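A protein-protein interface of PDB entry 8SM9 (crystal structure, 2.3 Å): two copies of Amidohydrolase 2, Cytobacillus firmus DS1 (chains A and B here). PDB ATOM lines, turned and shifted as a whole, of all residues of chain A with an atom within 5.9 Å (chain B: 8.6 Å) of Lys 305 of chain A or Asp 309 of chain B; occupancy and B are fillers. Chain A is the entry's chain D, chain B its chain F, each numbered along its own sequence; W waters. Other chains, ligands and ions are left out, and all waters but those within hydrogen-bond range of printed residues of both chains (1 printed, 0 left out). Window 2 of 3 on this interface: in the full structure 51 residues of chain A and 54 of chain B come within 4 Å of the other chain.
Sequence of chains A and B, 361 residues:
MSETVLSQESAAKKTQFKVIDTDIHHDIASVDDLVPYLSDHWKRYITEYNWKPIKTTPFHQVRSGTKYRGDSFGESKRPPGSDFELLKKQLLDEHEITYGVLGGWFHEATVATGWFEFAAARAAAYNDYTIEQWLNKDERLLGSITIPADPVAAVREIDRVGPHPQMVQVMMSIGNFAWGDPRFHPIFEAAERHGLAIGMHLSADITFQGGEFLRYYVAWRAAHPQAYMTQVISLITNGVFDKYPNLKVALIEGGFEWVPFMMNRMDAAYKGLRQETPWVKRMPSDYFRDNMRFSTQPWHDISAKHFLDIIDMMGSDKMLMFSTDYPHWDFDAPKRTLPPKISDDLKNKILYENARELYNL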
ATOM      1  N   SER A 303      -0.827 -27.183  17.528  1.00  0.00           N
ATOM      2  CA  SER A 303      -1.435 -28.502  17.508  1.00  0.00           C
ATOM      3  C   SER A 303      -0.448 -29.530  16.975  1.00  0.00           C
ATOM      4  O   SER A 303       0.475 -29.204  16.220  1.00  0.00           O
ATOM      5  CB  SER A 303      -2.689 -28.482  16.641  1.00  0.00           C
ATOM      6  OG  SER A 303      -2.338 -28.622  15.279  1.00  0.00           O
ATOM      7  N   ALA A 304      -0.641 -30.787  17.383  1.00  0.00           N
ATOM      8  CA  ALA A 304       0.201 -31.852  16.852  1.00  0.00           C
ATOM      9  C   ALA A 304      -0.097 -32.105  15.381  1.00  0.00           C
ATOM     10  O   ALA A 304       0.784 -32.560  14.640  1.00  0.00           O
ATOM     11  CB  ALA A 304       0.034 -33.135  17.667  1.00  0.00           C
ATOM     12  N   LYS A 305      -1.318 -31.803  14.932  1.00  0.00           N
ATOM     13  CA  LYS A 305      -1.585 -31.872  13.498  1.00  0.00           C
ATOM     14  C   LYS A 305      -0.755 -30.826  12.758  1.00  0.00           C
ATOM     15  O   LYS A 305      -0.064 -31.148  11.782  1.00  0.00           O
ATOM     16  CB  LYS A 305      -3.087 -31.713  13.211  1.00  0.00           C
ATOM     17  CG  LYS A 305      -3.423 -31.420  11.728  1.00  0.00           C
ATOM     18  CD  LYS A 305      -3.113 -32.598  10.775  1.00  0.00           C
ATOM     19  CE  LYS A 305      -3.192 -32.178   9.294  1.00  0.00           C
ATOM     20  NZ  LYS A 305      -2.365 -33.015   8.349  1.00  0.00           N
ATOM     21  N   HIS A 306      -0.741 -29.580  13.260  1.00  0.00           N
ATOM     22  CA  HIS A 306      -0.025 -28.511  12.562  1.00  0.00           C
ATOM     23  C   HIS A 306       1.492 -28.676  12.673  1.00  0.00           C
ATOM     24  O   HIS A 306       2.212 -28.418  11.705  1.00  0.00           O
ATOM     25  CB  HIS A 306      -0.484 -27.145  13.071  1.00  0.00           C
ATOM     26  CG  HIS A 306      -1.848 -26.752  12.580  1.00  0.00           C
ATOM     27  ND1 HIS A 306      -2.582 -25.728  13.144  1.00  0.00           N
ATOM     28  CD2 HIS A 306      -2.616 -27.256  11.579  1.00  0.00           C
ATOM     29  CE1 HIS A 306      -3.739 -25.616  12.512  1.00  0.00           C
ATOM     30  NE2 HIS A 306      -3.785 -26.530  11.559  1.00  0.00           N
ATOM     31  N   PHE A 307       1.995 -29.136  13.826  1.00  0.00           N
ATOM     32  CA  PHE A 307       3.425 -29.410  13.961  1.00  0.00           C
ATOM     33  C   PHE A 307       3.889 -30.451  12.949  1.00  0.00           C
ATOM     34  O   PHE A 307       4.927 -30.280  12.297  1.00  0.00           O
ATOM     35  CB  PHE A 307       3.729 -29.878  15.383  1.00  0.00           C
ATOM     36  CG  PHE A 307       5.202 -30.014  15.688  1.00  0.00           C
ATOM     37  CD1 PHE A 307       6.069 -28.945  15.518  1.00  0.00           C
ATOM     38  CD2 PHE A 307       5.715 -31.204  16.188  1.00  0.00           C
ATOM     39  CE1 PHE A 307       7.427 -29.068  15.821  1.00  0.00           C
ATOM     40  CE2 PHE A 307       7.069 -31.338  16.490  1.00  0.00           C
ATOM     41  CZ  PHE A 307       7.924 -30.271  16.304  1.00  0.00           C
ATOM     42  N   LEU A 308       3.125 -31.540  12.793  1.00  0.00           N
ATOM     43  CA  LEU A 308       3.541 -32.609  11.887  1.00  0.00           C
ATOM     44  C   LEU A 308       3.469 -32.167  10.433  1.00  0.00           C
ATOM     45  O   LEU A 308       4.318 -32.554   9.618  1.00  0.00           O
ATOM     46  CB  LEU A 308       2.694 -33.844  12.126  1.00  0.00           C
ATOM     47  CG  LEU A 308       2.983 -34.423  13.503  1.00  0.00           C
ATOM     48  CD1 LEU A 308       2.045 -35.568  13.752  1.00  0.00           C
ATOM     49  CD2 LEU A 308       4.431 -34.865  13.608  1.00  0.00           C
ATOM     50  N   ASP A 309       2.467 -31.353  10.091  1.00  0.00           N
ATOM     51  CA  ASP A 309       2.476 -30.684   8.794  1.00  0.00           C
ATOM     52  C   ASP A 309       3.798 -29.962   8.558  1.00  0.00           C
ATOM     53  O   ASP A 309       4.430 -30.123   7.509  1.00  0.00           O
ATOM     54  CB  ASP A 309       1.313 -29.698   8.704  1.00  0.00           C
ATOM     55  CG  ASP A 309      -0.038 -30.378   8.774  1.00  0.00           C
ATOM     56  OD1 ASP A 309      -0.182 -31.512   8.234  1.00  0.00           O
ATOM     57  OD2 ASP A 309      -0.954 -29.767   9.371  1.00  0.00           O
ATOM     58  N   ILE A 310       4.249 -29.187   9.553  1.00  0.00           N
ATOM     59  CA  ILE A 310       5.438 -28.363   9.384  1.00  0.00           C
ATOM     60  C   ILE A 310       6.672 -29.232   9.196  1.00  0.00           C
ATOM     61  O   ILE A 310       7.509 -28.955   8.331  1.00  0.00           O
ATOM     62  CB  ILE A 310       5.582 -27.394  10.568  1.00  0.00           C
ATOM     63  CG1 ILE A 310       4.421 -26.404  10.549  1.00  0.00           C
ATOM     64  CG2 ILE A 310       6.859 -26.630  10.469  1.00  0.00           C
ATOM     65  CD1 ILE A 310       4.333 -25.503  11.770  1.00  0.00           C
ATOM     66  N   MET A 313       6.444 -30.376   5.653  1.00  0.00           N
ATOM     67  CA  MET A 313       6.892 -29.298   4.761  1.00  0.00           C
ATOM     68  C   MET A 313       8.388 -29.073   4.835  1.00  0.00           C
ATOM     69  O   MET A 313       8.965 -28.456   3.942  1.00  0.00           O
ATOM     70  CB  MET A 313       6.185 -27.983   5.080  1.00  0.00           C
ATOM     71  CG  MET A 313       4.724 -28.006   4.791  1.00  0.00           C
ATOM     72  SD  MET A 313       3.904 -26.679   5.652  1.00  0.00           S
ATOM     73  CE  MET A 313       2.293 -26.615   4.887  1.00  0.00           C
ATOM     74  N   PHE B 256       2.698 -15.705   0.769  1.00  0.00           N
ATOM     75  CA  PHE B 256       1.755 -15.976   1.852  1.00  0.00           C
ATOM     76  C   PHE B 256       2.156 -17.143   2.756  1.00  0.00           C
ATOM     77  O   PHE B 256       1.600 -17.260   3.852  1.00  0.00           O
ATOM     78  CB  PHE B 256       0.361 -16.258   1.270  1.00  0.00           C
ATOM     79  CG  PHE B 256       0.306 -17.534   0.488  1.00  0.00           C
ATOM     80  CD1 PHE B 256       0.684 -17.551  -0.847  1.00  0.00           C
ATOM     81  CD2 PHE B 256      -0.063 -18.734   1.103  1.00  0.00           C
ATOM     82  CE1 PHE B 256       0.671 -18.753  -1.573  1.00  0.00           C
ATOM     83  CE2 PHE B 256      -0.069 -19.924   0.392  1.00  0.00           C
ATOM     84  CZ  PHE B 256       0.298 -19.935  -0.946  1.00  0.00           C
ATOM     85  N   PRO B 260       0.998 -17.979   8.305  1.00  0.00           N
ATOM     86  CA  PRO B 260       0.726 -18.724   9.521  1.00  0.00           C
ATOM     87  C   PRO B 260       1.758 -18.478  10.635  1.00  0.00           C
ATOM     88  O   PRO B 260       1.356 -18.321  11.760  1.00  0.00           O
ATOM     89  CB  PRO B 260       0.716 -20.180   9.042  1.00  0.00           C
ATOM     90  CG  PRO B 260       1.476 -20.168   7.745  1.00  0.00           C
ATOM     91  CD  PRO B 260       1.080 -18.851   7.125  1.00  0.00           C
ATOM     92  N   ILE B 302       3.380 -26.241  -5.064  1.00  0.00           N
ATOM     93  CA  ILE B 302       3.040 -26.613  -3.702  1.00  0.00           C
ATOM     94  C   ILE B 302       2.042 -27.758  -3.788  1.00  0.00           C
ATOM     95  O   ILE B 302       1.140 -27.758  -4.638  1.00  0.00           O
ATOM     96  CB  ILE B 302       2.518 -25.390  -2.904  1.00  0.00           C
ATOM     97  CG1 ILE B 302       2.825 -25.520  -1.419  1.00  0.00           C
ATOM     98  CG2 ILE B 302       1.051 -25.207  -3.066  1.00  0.00           C
ATOM     99  CD1 ILE B 302       2.272 -24.364  -0.610  1.00  0.00           C
ATOM    100  N   SER B 303       2.257 -28.778  -2.969  1.00  0.00           N
ATOM    101  CA  SER B 303       1.366 -29.916  -3.046  1.00  0.00           C
ATOM    102  C   SER B 303      -0.035 -29.492  -2.613  1.00  0.00           C
ATOM    103  O   SER B 303      -0.224 -28.482  -1.929  1.00  0.00           O
ATOM    104  CB  SER B 303       1.916 -31.071  -2.203  1.00  0.00           C
ATOM    105  OG  SER B 303       1.497 -31.003  -0.851  1.00  0.00           O
ATOM    106  N   ALA B 304      -1.032 -30.244  -3.069  1.00  0.00           N
ATOM    107  CA  ALA B 304      -2.402 -29.938  -2.677  1.00  0.00           C
ATOM    108  C   ALA B 304      -2.537 -29.945  -1.164  1.00  0.00           C
ATOM    109  O   ALA B 304      -3.151 -29.042  -0.578  1.00  0.00           O
ATOM    110  CB  ALA B 304      -3.372 -30.945  -3.295  1.00  0.00           C
ATOM    111  N   LYS B 305      -1.949 -30.945  -0.512  1.00  0.00           N
ATOM    112  CA  LYS B 305      -2.135 -31.090   0.922  1.00  0.00           C
ATOM    113  C   LYS B 305      -1.404 -29.987   1.687  1.00  0.00           C
ATOM    114  O   LYS B 305      -1.923 -29.461   2.680  1.00  0.00           O
ATOM    115  CB  LYS B 305      -1.667 -32.480   1.351  1.00  0.00           C
ATOM    116  CG  LYS B 305      -1.168 -32.573   2.770  1.00  0.00           C
ATOM    117  CD  LYS B 305      -0.508 -33.914   2.999  1.00  0.00           C
ATOM    118  CE  LYS B 305       0.926 -33.769   3.439  1.00  0.00           C
ATOM    119  NZ  LYS B 305       1.576 -35.100   3.399  1.00  0.00           N
ATOM    120  N   HIS B 306      -0.205 -29.608   1.228  1.00  0.00           N
ATOM    121  CA  HIS B 306       0.531 -28.534   1.886  1.00  0.00           C
ATOM    122  C   HIS B 306      -0.192 -27.206   1.730  1.00  0.00           C
ATOM    123  O   HIS B 306      -0.234 -26.401   2.668  1.00  0.00           O
ATOM    124  CB  HIS B 306       1.937 -28.434   1.313  1.00  0.00           C
ATOM    125  CG  HIS B 306       2.857 -29.491   1.806  1.00  0.00           C
ATOM    126  ND1 HIS B 306       4.019 -29.833   1.146  1.00  0.00           N
ATOM    127  CD2 HIS B 306       2.779 -30.300   2.894  1.00  0.00           C
ATOM    128  CE1 HIS B 306       4.624 -30.805   1.813  1.00  0.00           C
ATOM    129  NE2 HIS B 306       3.895 -31.103   2.880  1.00  0.00           N
ATOM    130  N   PHE B 307      -0.765 -26.959   0.551  1.00  0.00           N
ATOM    131  CA  PHE B 307      -1.561 -25.756   0.357  1.00  0.00           C
ATOM    132  C   PHE B 307      -2.765 -25.748   1.290  1.00  0.00           C
ATOM    133  O   PHE B 307      -3.009 -24.769   2.003  1.00  0.00           O
ATOM    134  CB  PHE B 307      -1.987 -25.653  -1.104  1.00  0.00           C
ATOM    135  CG  PHE B 307      -2.656 -24.366  -1.450  1.00  0.00           C
ATOM    136  CD1 PHE B 307      -1.990 -23.157  -1.294  1.00  0.00           C
ATOM    137  CD2 PHE B 307      -3.960 -24.359  -1.935  1.00  0.00           C
ATOM    138  CE1 PHE B 307      -2.610 -21.957  -1.624  1.00  0.00           C
ATOM    139  CE2 PHE B 307      -4.589 -23.168  -2.268  1.00  0.00           C
ATOM    140  CZ  PHE B 307      -3.912 -21.960  -2.109  1.00  0.00           C
ATOM    141  N   LEU B 308      -3.507 -26.856   1.341  1.00  0.00           N
ATOM    142  CA  LEU B 308      -4.647 -26.929   2.253  1.00  0.00           C
ATOM    143  C   LEU B 308      -4.211 -26.884   3.718  1.00  0.00           C
ATOM    144  O   LEU B 308      -4.950 -26.386   4.573  1.00  0.00           O
ATOM    145  CB  LEU B 308      -5.468 -28.184   1.941  1.00  0.00           C
ATOM    146  CG  LEU B 308      -5.999 -28.139   0.489  1.00  0.00           C
ATOM    147  CD1 LEU B 308      -6.563 -29.467   0.028  1.00  0.00           C
ATOM    148  CD2 LEU B 308      -7.016 -27.020   0.274  1.00  0.00           C
ATOM    149  N   ASP B 309      -3.008 -27.368   4.031  1.00  0.00           N
ATOM    150  CA  ASP B 309      -2.534 -27.234   5.399  1.00  0.00           C
ATOM    151  C   ASP B 309      -2.240 -25.775   5.729  1.00  0.00           C
ATOM    152  O   ASP B 309      -2.529 -25.311   6.842  1.00  0.00           O
ATOM    153  CB  ASP B 309      -1.303 -28.101   5.617  1.00  0.00           C
ATOM    154  CG  ASP B 309      -1.642 -29.562   5.755  1.00  0.00           C
ATOM    155  OD1 ASP B 309      -2.601 -29.922   6.484  1.00  0.00           O
ATOM    156  OD2 ASP B 309      -0.940 -30.360   5.111  1.00  0.00           O
ATOM    157  N   ILE B 310      -1.738 -25.008   4.767  1.00  0.00           N
ATOM    158  CA  ILE B 310      -1.502 -23.556   5.019  1.00  0.00           C
ATOM    159  C   ILE B 310      -2.841 -22.855   5.286  1.00  0.00           C
ATOM    160  O   ILE B 310      -2.880 -22.018   6.191  1.00  0.00           O
ATOM    161  CB  ILE B 310      -0.698 -22.914   3.871  1.00  0.00           C
ATOM    162  CG1 ILE B 310       0.678 -23.565   3.729  1.00  0.00           C
ATOM    163  CG2 ILE B 310      -0.588 -21.413   4.054  1.00  0.00           C
ATOM    164  CD1 ILE B 310       1.575 -22.891   2.726  1.00  0.00           C
ATOM    165  N   ILE B 311      -3.895 -23.206   4.548  1.00  0.00           N
ATOM    166  CA  ILE B 311      -5.208 -22.515   4.702  1.00  0.00           C
ATOM    167  C   ILE B 311      -5.830 -22.923   6.034  1.00  0.00           C
ATOM    168  O   ILE B 311      -6.406 -22.058   6.703  1.00  0.00           O
ATOM    169  CB  ILE B 311      -6.141 -22.818   3.517  1.00  0.00           C
ATOM    170  CG1 ILE B 311      -5.815 -21.939   2.307  1.00  0.00           C
ATOM    171  CG2 ILE B 311      -7.599 -22.690   3.922  1.00  0.00           C
ATOM    172  CD1 ILE B 311      -5.395 -22.715   1.087  1.00  0.00           C
ATOM    173  N   ASP B 312      -5.713 -24.199   6.397  1.00  0.00           N
ATOM    174  CA  ASP B 312      -6.222 -24.640   7.717  1.00  0.00           C
ATOM    175  C   ASP B 312      -5.473 -23.856   8.781  1.00  0.00           C
ATOM    176  O   ASP B 312      -6.097 -23.406   9.744  1.00  0.00           O
ATOM    177  CB  ASP B 312      -6.043 -26.136   7.936  1.00  0.00           C
ATOM    178  CG  ASP B 312      -6.593 -26.610   9.267  1.00  0.00           C
ATOM    179  OD1 ASP B 312      -7.759 -26.302   9.558  1.00  0.00           O
ATOM    180  OD2 ASP B 312      -5.850 -27.282   9.996  1.00  0.00           O
ATOM    181  N   MET B 313      -4.166 -23.714   8.586  1.00  0.00           N
ATOM    182  CA  MET B 313      -3.388 -22.986   9.581  1.00  0.00           C
ATOM    183  C   MET B 313      -3.843 -21.533   9.676  1.00  0.00           C
ATOM    184  O   MET B 313      -3.706 -20.893  10.721  1.00  0.00           O
ATOM    185  CB  MET B 313      -1.912 -23.096   9.219  1.00  0.00           C
ATOM    186  CG  MET B 313      -1.221 -24.248   9.895  1.00  0.00           C
ATOM    187  SD  MET B 313       0.472 -24.669   9.403  1.00  0.00           S
ATOM    188  CE  MET B 313       0.412 -24.499   7.650  1.00  0.00           C
ATOM    189  N   MET B 314      -4.416 -21.001   8.609  1.00  0.00           N
ATOM    190  CA  MET B 314      -4.811 -19.607   8.660  1.00  0.00           C
ATOM    191  C   MET B 314      -6.138 -19.436   9.372  1.00  0.00           C
ATOM    192  O   MET B 314      -6.398 -18.375   9.940  1.00  0.00           O
ATOM    193  CB  MET B 314      -4.859 -19.026   7.242  1.00  0.00           C
ATOM    194  CG  MET B 314      -3.490 -18.954   6.506  1.00  0.00           C
ATOM    195  SD  MET B 314      -3.704 -18.122   4.910  1.00  0.00           S
ATOM    196  CE  MET B 314      -2.210 -18.450   4.012  1.00  0.00           C
ATOM    197  N   GLY B 315      -6.983 -20.459   9.381  1.00  0.00           N
ATOM    198  CA  GLY B 315      -8.260 -20.305  10.022  1.00  0.00           C
ATOM    199  C   GLY B 315      -9.295 -19.602   9.187  1.00  0.00           C
ATOM    200  O   GLY B 315     -10.369 -19.278   9.706  1.00  0.00           O
ATOM    201  N   ILE B 342      -7.632 -28.851  -5.965  1.00  0.00           N
ATOM    202  CA  ILE B 342      -8.434 -28.169  -4.952  1.00  0.00           C
ATOM    203  C   ILE B 342      -9.857 -27.996  -5.456  1.00  0.00           C
ATOM    204  O   ILE B 342     -10.132 -28.040  -6.660  1.00  0.00           O
ATOM    205  CB  ILE B 342      -7.859 -26.810  -4.509  1.00  0.00           C
ATOM    206  CG1 ILE B 342      -7.627 -25.900  -5.706  1.00  0.00           C
ATOM    207  CG2 ILE B 342      -6.594 -26.984  -3.705  1.00  0.00           C
ATOM    208  CD1 ILE B 342      -7.292 -24.497  -5.273  1.00  0.00           C
ATOM    209  N   LEU B 346     -12.868 -23.388  -3.421  1.00  0.00           N
ATOM    210  CA  LEU B 346     -11.663 -22.644  -3.055  1.00  0.00           C
ATOM    211  C   LEU B 346     -11.028 -21.980  -4.275  1.00  0.00           C
ATOM    212  O   LEU B 346     -10.551 -20.844  -4.184  1.00  0.00           O
ATOM    213  CB  LEU B 346     -10.670 -23.573  -2.362  1.00  0.00           C
ATOM    214  CG  LEU B 346      -9.467 -22.991  -1.647  1.00  0.00           C
ATOM    215  CD1 LEU B 346      -9.884 -21.944  -0.602  1.00  0.00           C
ATOM    216  CD2 LEU B 346      -8.669 -24.133  -1.014  1.00  0.00           C
HETATM  217  O   HOH W   1      -4.009 -31.955   6.422  1.00  0.00           O
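Lys 305 of chain A touches Asp 309 of chain B, but with the chains exchanged Asp 309 of chain A does not touch Lys 305 of chain B (5.4 Å). His 306 of chain A touches Met 313 of chain B, and with the chains exchanged Met 313 of chain A touches His 306 of chain B. Met 313 of chain A touches Asp 309 of chain B, but with the chains exchanged Asp 309 of chain A does not touch Met 313 of chain B (5.1 Å). Met 313 of chain A touches Ile 310 of chain B, but with the chains exchanged Ile 310 of chain A does not touch Met 313 of chain B (4.5 Å). Positions printed for both chains: 303, 304, 305, 306, 307, 308, 309, 310 and 313.
Hydrophobic or aromatic side chains of chain A within 4 Å of the printed part of chain B: His 306 and Met 313. Among the printed residues, Asp or Glu carboxylates within 4 Å of a Lys or Arg side-chain nitrogen of the other chain: Lys 305 of chain A with Asp 309 of chain B (3.6 Å).
Of the printed residues of chain B, Met 313 of chain A touches His 306, Asp 309, Ile 310 and Met 313. Asp 309 of chain B touches just these residues of chain A: Lys 305, Asp 309 and Met 313. Printed residues of chain A within 4 Å of Asp 312 of chain B: His 306. The nearest residue of chain A that does not touch Asp 309 of chain B is His 306 of chain A (5.0 Å). The nearest printed residue of chain A that does not touch Ile 310 of chain B is Asp 309 of chain A (6.7 Å).
N of His 306 of chain A is in hydrogen-bond range of OG of Ser 303 of chain A, 2.7 Å away. OG of Ser 303 of chain A lies close to N of Lys 305 of chain A (3.4 Å). The side-chain amino group of Lys 305 of chain A is in salt-bridge range of the side-chain carboxylate of Asp 309 of chain A (2.7 Å). OG of Ser 303 of chain B is in hydrogen-bond range of N of His 306 of chain B (3.0 Å).
Water W1 lies within hydrogen-bond range of the side-chain carboxylate (OD1) of Asp 309 of chain B and the side-chain amino group (NZ) of Lys 305 of chain A.
The side-chain carboxylate of Asp 312 of chain B lies within hydrogen-bond range of a ring nitrogen (NE2) of His 306 of chain A (2.7 Å). The side-chain carboxylate (OD2) of Asp 309 of chain A sits close to the side-chain carboxylate (OD1) of Asp 309 of chain B (3.3 Å). OD1 of Asp 309 of chain B is in salt-bridge range of NZ of Lys 305 of chain A, 3.6 Å away.
His 306 of chain A touches Met 313 of chain B (CD2 to CG, 3.7 Å). Met 313 of chain A touches His 306 of chain B (CE to O, 3.4 Å). CE of Met 313 of chain A touches CB of Asp 309 of chain B (3.96 Å). CE of Met 313 of chain A touches CG1 of Ile 310 of chain B (3.6 Å). Met 313 of chain B touches Met 313 of chain A.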
